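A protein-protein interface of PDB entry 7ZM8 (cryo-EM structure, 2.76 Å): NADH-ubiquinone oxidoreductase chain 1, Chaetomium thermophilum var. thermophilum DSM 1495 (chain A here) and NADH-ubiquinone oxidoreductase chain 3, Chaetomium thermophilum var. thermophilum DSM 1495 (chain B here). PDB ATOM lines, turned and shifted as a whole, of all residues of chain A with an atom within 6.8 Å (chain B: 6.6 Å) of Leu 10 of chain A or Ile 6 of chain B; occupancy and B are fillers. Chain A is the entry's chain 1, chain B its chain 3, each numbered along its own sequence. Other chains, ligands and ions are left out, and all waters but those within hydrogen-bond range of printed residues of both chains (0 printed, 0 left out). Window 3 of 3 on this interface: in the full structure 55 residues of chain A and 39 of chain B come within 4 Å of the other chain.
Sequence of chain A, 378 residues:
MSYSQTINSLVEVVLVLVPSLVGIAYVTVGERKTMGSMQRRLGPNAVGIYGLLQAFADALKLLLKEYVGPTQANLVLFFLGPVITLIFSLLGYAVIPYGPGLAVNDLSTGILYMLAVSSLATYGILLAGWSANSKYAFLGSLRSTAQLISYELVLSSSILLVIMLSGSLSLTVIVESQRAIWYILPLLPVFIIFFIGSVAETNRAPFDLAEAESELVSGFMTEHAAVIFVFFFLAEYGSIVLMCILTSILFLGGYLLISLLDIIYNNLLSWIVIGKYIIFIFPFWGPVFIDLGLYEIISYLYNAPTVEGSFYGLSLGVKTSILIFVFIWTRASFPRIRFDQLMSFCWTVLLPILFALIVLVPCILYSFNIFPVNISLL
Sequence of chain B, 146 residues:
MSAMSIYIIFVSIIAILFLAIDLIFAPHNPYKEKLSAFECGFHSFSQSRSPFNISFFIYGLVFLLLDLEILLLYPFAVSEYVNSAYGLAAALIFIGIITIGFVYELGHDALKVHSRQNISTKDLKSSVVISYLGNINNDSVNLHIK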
ATOM      1  N   GLN A   5      -1.933  35.416  -6.081  1.00  0.00           N
ATOM      2  CA  GLN A   5      -2.782  34.470  -5.328  1.00  0.00           C
ATOM      3  C   GLN A   5      -3.915  33.974  -6.216  1.00  0.00           C
ATOM      4  O   GLN A   5      -4.243  32.815  -6.128  1.00  0.00           O
ATOM      5  CB  GLN A   5      -3.332  35.187  -4.098  1.00  0.00           C
ATOM      6  CG  GLN A   5      -3.085  34.437  -2.802  1.00  0.00           C
ATOM      7  CD  GLN A   5      -3.306  35.334  -1.613  1.00  0.00           C
ATOM      8  OE1 GLN A   5      -3.787  36.455  -1.744  1.00  0.00           O
ATOM      9  NE2 GLN A   5      -2.950  34.842  -0.437  1.00  0.00           N
ATOM     10  N   THR A   6      -4.489  34.841  -7.030  1.00  0.00           N
ATOM     11  CA  THR A   6      -5.646  34.463  -7.868  1.00  0.00           C
ATOM     12  C   THR A   6      -5.242  33.344  -8.812  1.00  0.00           C
ATOM     13  O   THR A   6      -6.036  32.411  -8.955  1.00  0.00           O
ATOM     14  CB  THR A   6      -6.096  35.646  -8.727  1.00  0.00           C
ATOM     15  OG1 THR A   6      -6.344  36.755  -7.863  1.00  0.00           O
ATOM     16  CG2 THR A   6      -7.332  35.355  -9.548  1.00  0.00           C
ATOM     17  N   ILE A   7      -4.065  33.432  -9.429  1.00  0.00           N
ATOM     18  CA  ILE A   7      -3.582  32.315 -10.281  1.00  0.00           C
ATOM     19  C   ILE A   7      -3.427  31.083  -9.393  1.00  0.00           C
ATOM     20  O   ILE A   7      -3.941  30.036  -9.773  1.00  0.00           O
ATOM     21  CB  ILE A   7      -2.284  32.692 -11.011  1.00  0.00           C
ATOM     22  CG1 ILE A   7      -2.499  33.863 -11.973  1.00  0.00           C
ATOM     23  CG2 ILE A   7      -1.678  31.490 -11.715  1.00  0.00           C
ATOM     24  CD1 ILE A   7      -3.470  33.568 -13.089  1.00  0.00           C
ATOM     25  N   ASN A   8      -2.731  31.194  -8.262  1.00  0.00           N
ATOM     26  CA  ASN A   8      -2.532  30.046  -7.350  1.00  0.00           C
ATOM     27  C   ASN A   8      -3.890  29.404  -7.084  1.00  0.00           C
ATOM     28  O   ASN A   8      -3.988  28.180  -7.155  1.00  0.00           O
ATOM     29  CB  ASN A   8      -1.866  30.459  -6.036  1.00  0.00           C
ATOM     30  CG  ASN A   8      -1.493  29.292  -5.145  1.00  0.00           C
ATOM     31  OD1 ASN A   8      -0.692  28.442  -5.519  1.00  0.00           O
ATOM     32  ND2 ASN A   8      -2.054  29.259  -3.951  1.00  0.00           N
ATOM     33  N   SER A   9      -4.874  30.205  -6.708  1.00  0.00           N
ATOM     34  CA  SER A   9      -6.211  29.679  -6.349  1.00  0.00           C
ATOM     35  C   SER A   9      -6.804  28.903  -7.521  1.00  0.00           C
ATOM     36  O   SER A   9      -7.264  27.788  -7.294  1.00  0.00           O
ATOM     37  CB  SER A   9      -7.091  30.810  -5.926  1.00  0.00           C
ATOM     38  OG  SER A   9      -6.540  31.481  -4.806  1.00  0.00           O
ATOM     39  N   LEU A  10      -6.772  29.473  -8.723  1.00  0.00           N
ATOM     40  CA  LEU A  10      -7.366  28.824  -9.909  1.00  0.00           C
ATOM     41  C   LEU A  10      -6.642  27.522 -10.217  1.00  0.00           C
ATOM     42  O   LEU A  10      -7.319  26.545 -10.499  1.00  0.00           O
ATOM     43  CB  LEU A  10      -7.256  29.812 -11.069  1.00  0.00           C
ATOM     44  CG  LEU A  10      -8.511  30.627 -11.367  1.00  0.00           C
ATOM     45  CD1 LEU A  10      -8.172  31.834 -12.225  1.00  0.00           C
ATOM     46  CD2 LEU A  10      -9.554  29.762 -12.055  1.00  0.00           C
ATOM     47  N   VAL A  11      -5.317  27.527 -10.151  1.00  0.00           N
ATOM     48  CA  VAL A  11      -4.533  26.313 -10.495  1.00  0.00           C
ATOM     49  C   VAL A  11      -4.913  25.191  -9.525  1.00  0.00           C
ATOM     50  O   VAL A  11      -5.174  24.078  -9.990  1.00  0.00           O
ATOM     51  CB  VAL A  11      -3.027  26.604 -10.499  1.00  0.00           C
ATOM     52  CG1 VAL A  11      -2.222  25.344 -10.764  1.00  0.00           C
ATOM     53  CG2 VAL A  11      -2.676  27.674 -11.518  1.00  0.00           C
ATOM     54  N   GLU A  12      -5.018  25.493  -8.233  1.00  0.00           N
ATOM     55  CA  GLU A  12      -5.403  24.473  -7.232  1.00  0.00           C
ATOM     56  C   GLU A  12      -6.840  23.995  -7.442  1.00  0.00           C
ATOM     57  O   GLU A  12      -7.081  22.782  -7.370  1.00  0.00           O
ATOM     58  CB  GLU A  12      -5.125  24.979  -5.824  1.00  0.00           C
ATOM     59  CG  GLU A  12      -3.676  25.380  -5.634  1.00  0.00           C
ATOM     60  CD  GLU A  12      -3.248  25.587  -4.195  1.00  0.00           C
ATOM     61  OE1 GLU A  12      -3.682  26.579  -3.590  1.00  0.00           O
ATOM     62  OE2 GLU A  12      -2.484  24.746  -3.689  1.00  0.00           O
ATOM     63  N   VAL A  13      -7.750  24.916  -7.715  1.00  0.00           N
ATOM     64  CA  VAL A  13      -9.176  24.546  -7.919  1.00  0.00           C
ATOM     65  C   VAL A  13      -9.337  23.641  -9.149  1.00  0.00           C
ATOM     66  O   VAL A  13     -10.075  22.654  -9.026  1.00  0.00           O
ATOM     67  CB  VAL A  13     -10.079  25.794  -7.975  1.00  0.00           C
ATOM     68  CG1 VAL A  13     -11.472  25.465  -8.487  1.00  0.00           C
ATOM     69  CG2 VAL A  13     -10.148  26.491  -6.627  1.00  0.00           C
ATOM     70  N   VAL A  14      -8.682  23.943 -10.273  1.00  0.00           N
ATOM     71  CA  VAL A  14      -8.731  23.064 -11.480  1.00  0.00           C
ATOM     72  C   VAL A  14      -8.011  21.736 -11.232  1.00  0.00           C
ATOM     73  O   VAL A  14      -8.494  20.716 -11.720  1.00  0.00           O
ATOM     74  CB  VAL A  14      -8.203  23.775 -12.736  1.00  0.00           C
ATOM     75  CG1 VAL A  14      -8.879  25.117 -12.959  1.00  0.00           C
ATOM     76  CG2 VAL A  14      -6.691  23.915 -12.746  1.00  0.00           C
ATOM     77  N   LEU A  15      -6.904  21.746 -10.482  1.00  0.00           N
ATOM     78  CA  LEU A  15      -6.084  20.519 -10.256  1.00  0.00           C
ATOM     79  C   LEU A  15      -6.821  19.559  -9.333  1.00  0.00           C
ATOM     80  O   LEU A  15      -6.433  18.398  -9.288  1.00  0.00           O
ATOM     81  CB  LEU A  15      -4.714  20.871  -9.666  1.00  0.00           C
ATOM     82  CG  LEU A  15      -3.562  20.956 -10.661  1.00  0.00           C
ATOM     83  CD1 LEU A  15      -2.374  21.666 -10.037  1.00  0.00           C
ATOM     84  CD2 LEU A  15      -3.164  19.572 -11.146  1.00  0.00           C
ATOM     85  N   VAL A  16      -7.805  20.057  -8.593  1.00  0.00           N
ATOM     86  CA  VAL A  16      -8.551  19.193  -7.643  1.00  0.00           C
ATOM     87  C   VAL A  16      -9.859  18.815  -8.303  1.00  0.00           C
ATOM     88  O   VAL A  16     -10.160  17.621  -8.358  1.00  0.00           O
ATOM     89  CB  VAL A  16      -8.825  19.917  -6.310  1.00  0.00           C
ATOM     90  CG1 VAL A  16     -10.005  19.323  -5.558  1.00  0.00           C
ATOM     91  CG2 VAL A  16      -7.604  19.947  -5.423  1.00  0.00           C
ATOM     92  N   MET B   1      -7.679  36.285  -5.480  1.00  0.00           N
ATOM     93  CA  MET B   1      -8.849  36.008  -4.604  1.00  0.00           C
ATOM     94  C   MET B   1      -8.573  34.741  -3.788  1.00  0.00           C
ATOM     95  O   MET B   1      -7.581  34.058  -4.095  1.00  0.00           O
ATOM     96  CB  MET B   1     -10.137  35.853  -5.418  1.00  0.00           C
ATOM     97  CG  MET B   1     -10.623  37.159  -6.013  1.00  0.00           C
ATOM     98  SD  MET B   1     -12.035  36.949  -7.126  1.00  0.00           S
ATOM     99  CE  MET B   1     -11.224  36.243  -8.559  1.00  0.00           C
ATOM    100  N   SER B   2      -9.456  34.424  -2.835  1.00  0.00           N
ATOM    101  CA  SER B   2      -9.291  33.201  -2.009  1.00  0.00           C
ATOM    102  C   SER B   2      -9.632  31.961  -2.839  1.00  0.00           C
ATOM    103  O   SER B   2     -10.441  32.074  -3.770  1.00  0.00           O
ATOM    104  CB  SER B   2     -10.129  33.261  -0.762  1.00  0.00           C
ATOM    105  OG  SER B   2     -11.428  32.745  -1.003  1.00  0.00           O
ATOM    106  N   ALA B   3      -9.024  30.826  -2.506  1.00  0.00           N
ATOM    107  CA  ALA B   3      -9.286  29.565  -3.215  1.00  0.00           C
ATOM    108  C   ALA B   3     -10.725  29.117  -2.998  1.00  0.00           C
ATOM    109  O   ALA B   3     -11.288  28.552  -3.923  1.00  0.00           O
ATOM    110  CB  ALA B   3      -8.323  28.543  -2.702  1.00  0.00           C
ATOM    111  N   MET B   4     -11.241  29.310  -1.782  1.00  0.00           N
ATOM    112  CA  MET B   4     -12.612  28.872  -1.433  1.00  0.00           C
ATOM    113  C   MET B   4     -13.564  29.608  -2.370  1.00  0.00           C
ATOM    114  O   MET B   4     -14.426  28.955  -2.959  1.00  0.00           O
ATOM    115  CB  MET B   4     -12.959  29.166   0.028  1.00  0.00           C
ATOM    116  CG  MET B   4     -14.107  28.328   0.542  1.00  0.00           C
ATOM    117  SD  MET B   4     -13.768  26.561   0.369  1.00  0.00           S
ATOM    118  CE  MET B   4     -15.436  25.910   0.382  1.00  0.00           C
ATOM    119  N   SER B   5     -13.370  30.917  -2.520  1.00  0.00           N
ATOM    120  CA  SER B   5     -14.291  31.718  -3.365  1.00  0.00           C
ATOM    121  C   SER B   5     -14.196  31.253  -4.821  1.00  0.00           C
ATOM    122  O   SER B   5     -15.242  30.955  -5.394  1.00  0.00           O
ATOM    123  CB  SER B   5     -13.984  33.182  -3.226  1.00  0.00           C
ATOM    124  OG  SER B   5     -12.650  33.463  -3.619  1.00  0.00           O
ATOM    125  N   ILE B   6     -12.991  31.165  -5.376  1.00  0.00           N
ATOM    126  CA  ILE B   6     -12.790  30.746  -6.794  1.00  0.00           C
ATOM    127  C   ILE B   6     -13.330  29.326  -6.985  1.00  0.00           C
ATOM    128  O   ILE B   6     -13.932  29.074  -8.028  1.00  0.00           O
ATOM    129  CB  ILE B   6     -11.319  30.930  -7.212  1.00  0.00           C
ATOM    130  CG1 ILE B   6     -10.926  32.408  -7.201  1.00  0.00           C
ATOM    131  CG2 ILE B   6     -11.042  30.285  -8.557  1.00  0.00           C
ATOM    132  CD1 ILE B   6      -9.552  32.679  -7.750  1.00  0.00           C
ATOM    133  N   TYR B   7     -13.180  28.457  -5.982  1.00  0.00           N
ATOM    134  CA  TYR B   7     -13.719  27.072  -6.039  1.00  0.00           C
ATOM    135  C   TYR B   7     -15.244  27.089  -6.155  1.00  0.00           C
ATOM    136  O   TYR B   7     -15.782  26.365  -6.997  1.00  0.00           O
ATOM    137  CB  TYR B   7     -13.323  26.298  -4.778  1.00  0.00           C
ATOM    138  CG  TYR B   7     -13.690  24.838  -4.792  1.00  0.00           C
ATOM    139  CD1 TYR B   7     -14.854  24.386  -4.193  1.00  0.00           C
ATOM    140  CD2 TYR B   7     -12.873  23.909  -5.411  1.00  0.00           C
ATOM    141  CE1 TYR B   7     -15.199  23.045  -4.208  1.00  0.00           C
ATOM    142  CE2 TYR B   7     -13.201  22.566  -5.436  1.00  0.00           C
ATOM    143  CZ  TYR B   7     -14.367  22.134  -4.832  1.00  0.00           C
ATOM    144  OH  TYR B   7     -14.690  20.812  -4.856  1.00  0.00           O
ATOM    145  N   ILE B   8     -15.914  27.875  -5.318  1.00  0.00           N
ATOM    146  CA  ILE B   8     -17.406  27.913  -5.304  1.00  0.00           C
ATOM    147  C   ILE B   8     -17.886  28.452  -6.644  1.00  0.00           C
ATOM    148  O   ILE B   8     -18.830  27.882  -7.191  1.00  0.00           O
ATOM    149  CB  ILE B   8     -17.932  28.743  -4.118  1.00  0.00           C
ATOM    150  CG1 ILE B   8     -17.350  28.251  -2.790  1.00  0.00           C
ATOM    151  CG2 ILE B   8     -19.452  28.758  -4.091  1.00  0.00           C
ATOM    152  CD1 ILE B   8     -17.824  29.027  -1.585  1.00  0.00           C
ATOM    153  N   ILE B   9     -17.220  29.481  -7.162  1.00  0.00           N
ATOM    154  CA  ILE B   9     -17.586  30.061  -8.482  1.00  0.00           C
ATOM    155  C   ILE B   9     -17.396  29.016  -9.582  1.00  0.00           C
ATOM    156  O   ILE B   9     -18.236  28.956 -10.469  1.00  0.00           O
ATOM    157  CB  ILE B   9     -16.726  31.312  -8.733  1.00  0.00           C
ATOM    158  CG1 ILE B   9     -17.006  32.403  -7.696  1.00  0.00           C
ATOM    159  CG2 ILE B   9     -16.912  31.836 -10.148  1.00  0.00           C
ATOM    160  CD1 ILE B   9     -18.448  32.849  -7.656  1.00  0.00           C
ATOM    161  N   PHE B  10     -16.301  28.262  -9.551  1.00  0.00           N
ATOM    162  CA  PHE B  10     -16.010  27.282 -10.622  1.00  0.00           C
ATOM    163  C   PHE B  10     -17.055  26.177 -10.590  1.00  0.00           C
ATOM    164  O   PHE B  10     -17.529  25.746 -11.651  1.00  0.00           O
ATOM    165  CB  PHE B  10     -14.595  26.728 -10.491  1.00  0.00           C
ATOM    166  CG  PHE B  10     -13.880  26.555 -11.806  1.00  0.00           C
ATOM    167  CD1 PHE B  10     -13.171  27.604 -12.367  1.00  0.00           C
ATOM    168  CD2 PHE B  10     -13.922  25.349 -12.484  1.00  0.00           C
ATOM    169  CE1 PHE B  10     -12.515  27.448 -13.577  1.00  0.00           C
ATOM    170  CE2 PHE B  10     -13.267  25.194 -13.695  1.00  0.00           C
ATOM    171  CZ  PHE B  10     -12.564  26.244 -14.238  1.00  0.00           C
ATOM    172  N   VAL B  11     -17.398  25.735  -9.387  1.00  0.00           N
ATOM    173  CA  VAL B  11     -18.435  24.678  -9.257  1.00  0.00           C
ATOM    174  C   VAL B  11     -19.730  25.286  -9.787  1.00  0.00           C
ATOM    175  O   VAL B  11     -20.439  24.598 -10.549  1.00  0.00           O
ATOM    176  CB  VAL B  11     -18.550  24.179  -7.803  1.00  0.00           C
ATOM    177  CG1 VAL B  11     -19.795  23.334  -7.594  1.00  0.00           C
ATOM    178  CG2 VAL B  11     -17.311  23.415  -7.369  1.00  0.00           C
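N of Met 1 of chain B is in hydrogen-bond range of OG1 of Thr 6 of chain A (2.8 Å). The side-chain hydroxyl of Ser 9 of chain A is in hydrogen-bond range of the backbone carbonyl oxygen of Met 1 of chain B, 2.9 Å away. The backbone NH of Ala 3 of chain B lies within hydrogen-bond range of the side-chain hydroxyl of Ser 9 of chain A (3.4 Å).
The backbone carbonyl oxygen (O) of Gln 5 of chain A lies within hydrogen-bond range of the side-chain hydroxyl (OG) of Ser 9 of chain A (3.0 Å). The backbone carbonyl oxygen (O) of Ser 2 of chain B lies within hydrogen-bond range of the side-chain hydroxyl (OG) of Ser 5 of chain B (2.6 Å).
Among the printed residues, merely in contact across the chains: Val 13 of chain A with Ala 3 of chain B (3.6 Å), Ser 9 of chain A with Ile 6 of chain B (3.6 Å), Val 13 of chain A with Tyr 7 of chain B (3.7 Å), Ser 9 of chain A with Ser 2 of chain B (3.7 Å), Thr 6 of chain A with Ile 6 of chain B (3.7 Å), Leu 10 of chain A with Ile 6 of chain B (3.8 Å) and Val 13 of chain A with Phe 10 of chain B (3.9 Å).
Of the printed residues of chain A, Ala 3 of chain B touches Ser 9 (3.4 Å) and Val 13 (3.6 Å). Of the printed residues of chain A, Met 1 of chain B touches Thr 6 and Ser 9. Asn 8 of chain A touches none of the printed residues of chain B. The nearest residue of chain B that does not touch Leu 10 of chain A is Phe 10 of chain B (4.1 Å). The nearest printed residue of chain A that does not touch Met 1 of chain B is Gln 5 of chain A (4.1 Å).
Of the 12 printed residues of chain A, 4 touch a printed residue of chain B. Of the 11 printed residues of chain B, 6 touch a printed residue of chain A. Hydrophobic or aromatic side chains of chain B that line the printed part of chain A: Ile 6, Tyr 7 and Phe 10. Among the printed residues, 10 pairs touch across the chains.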
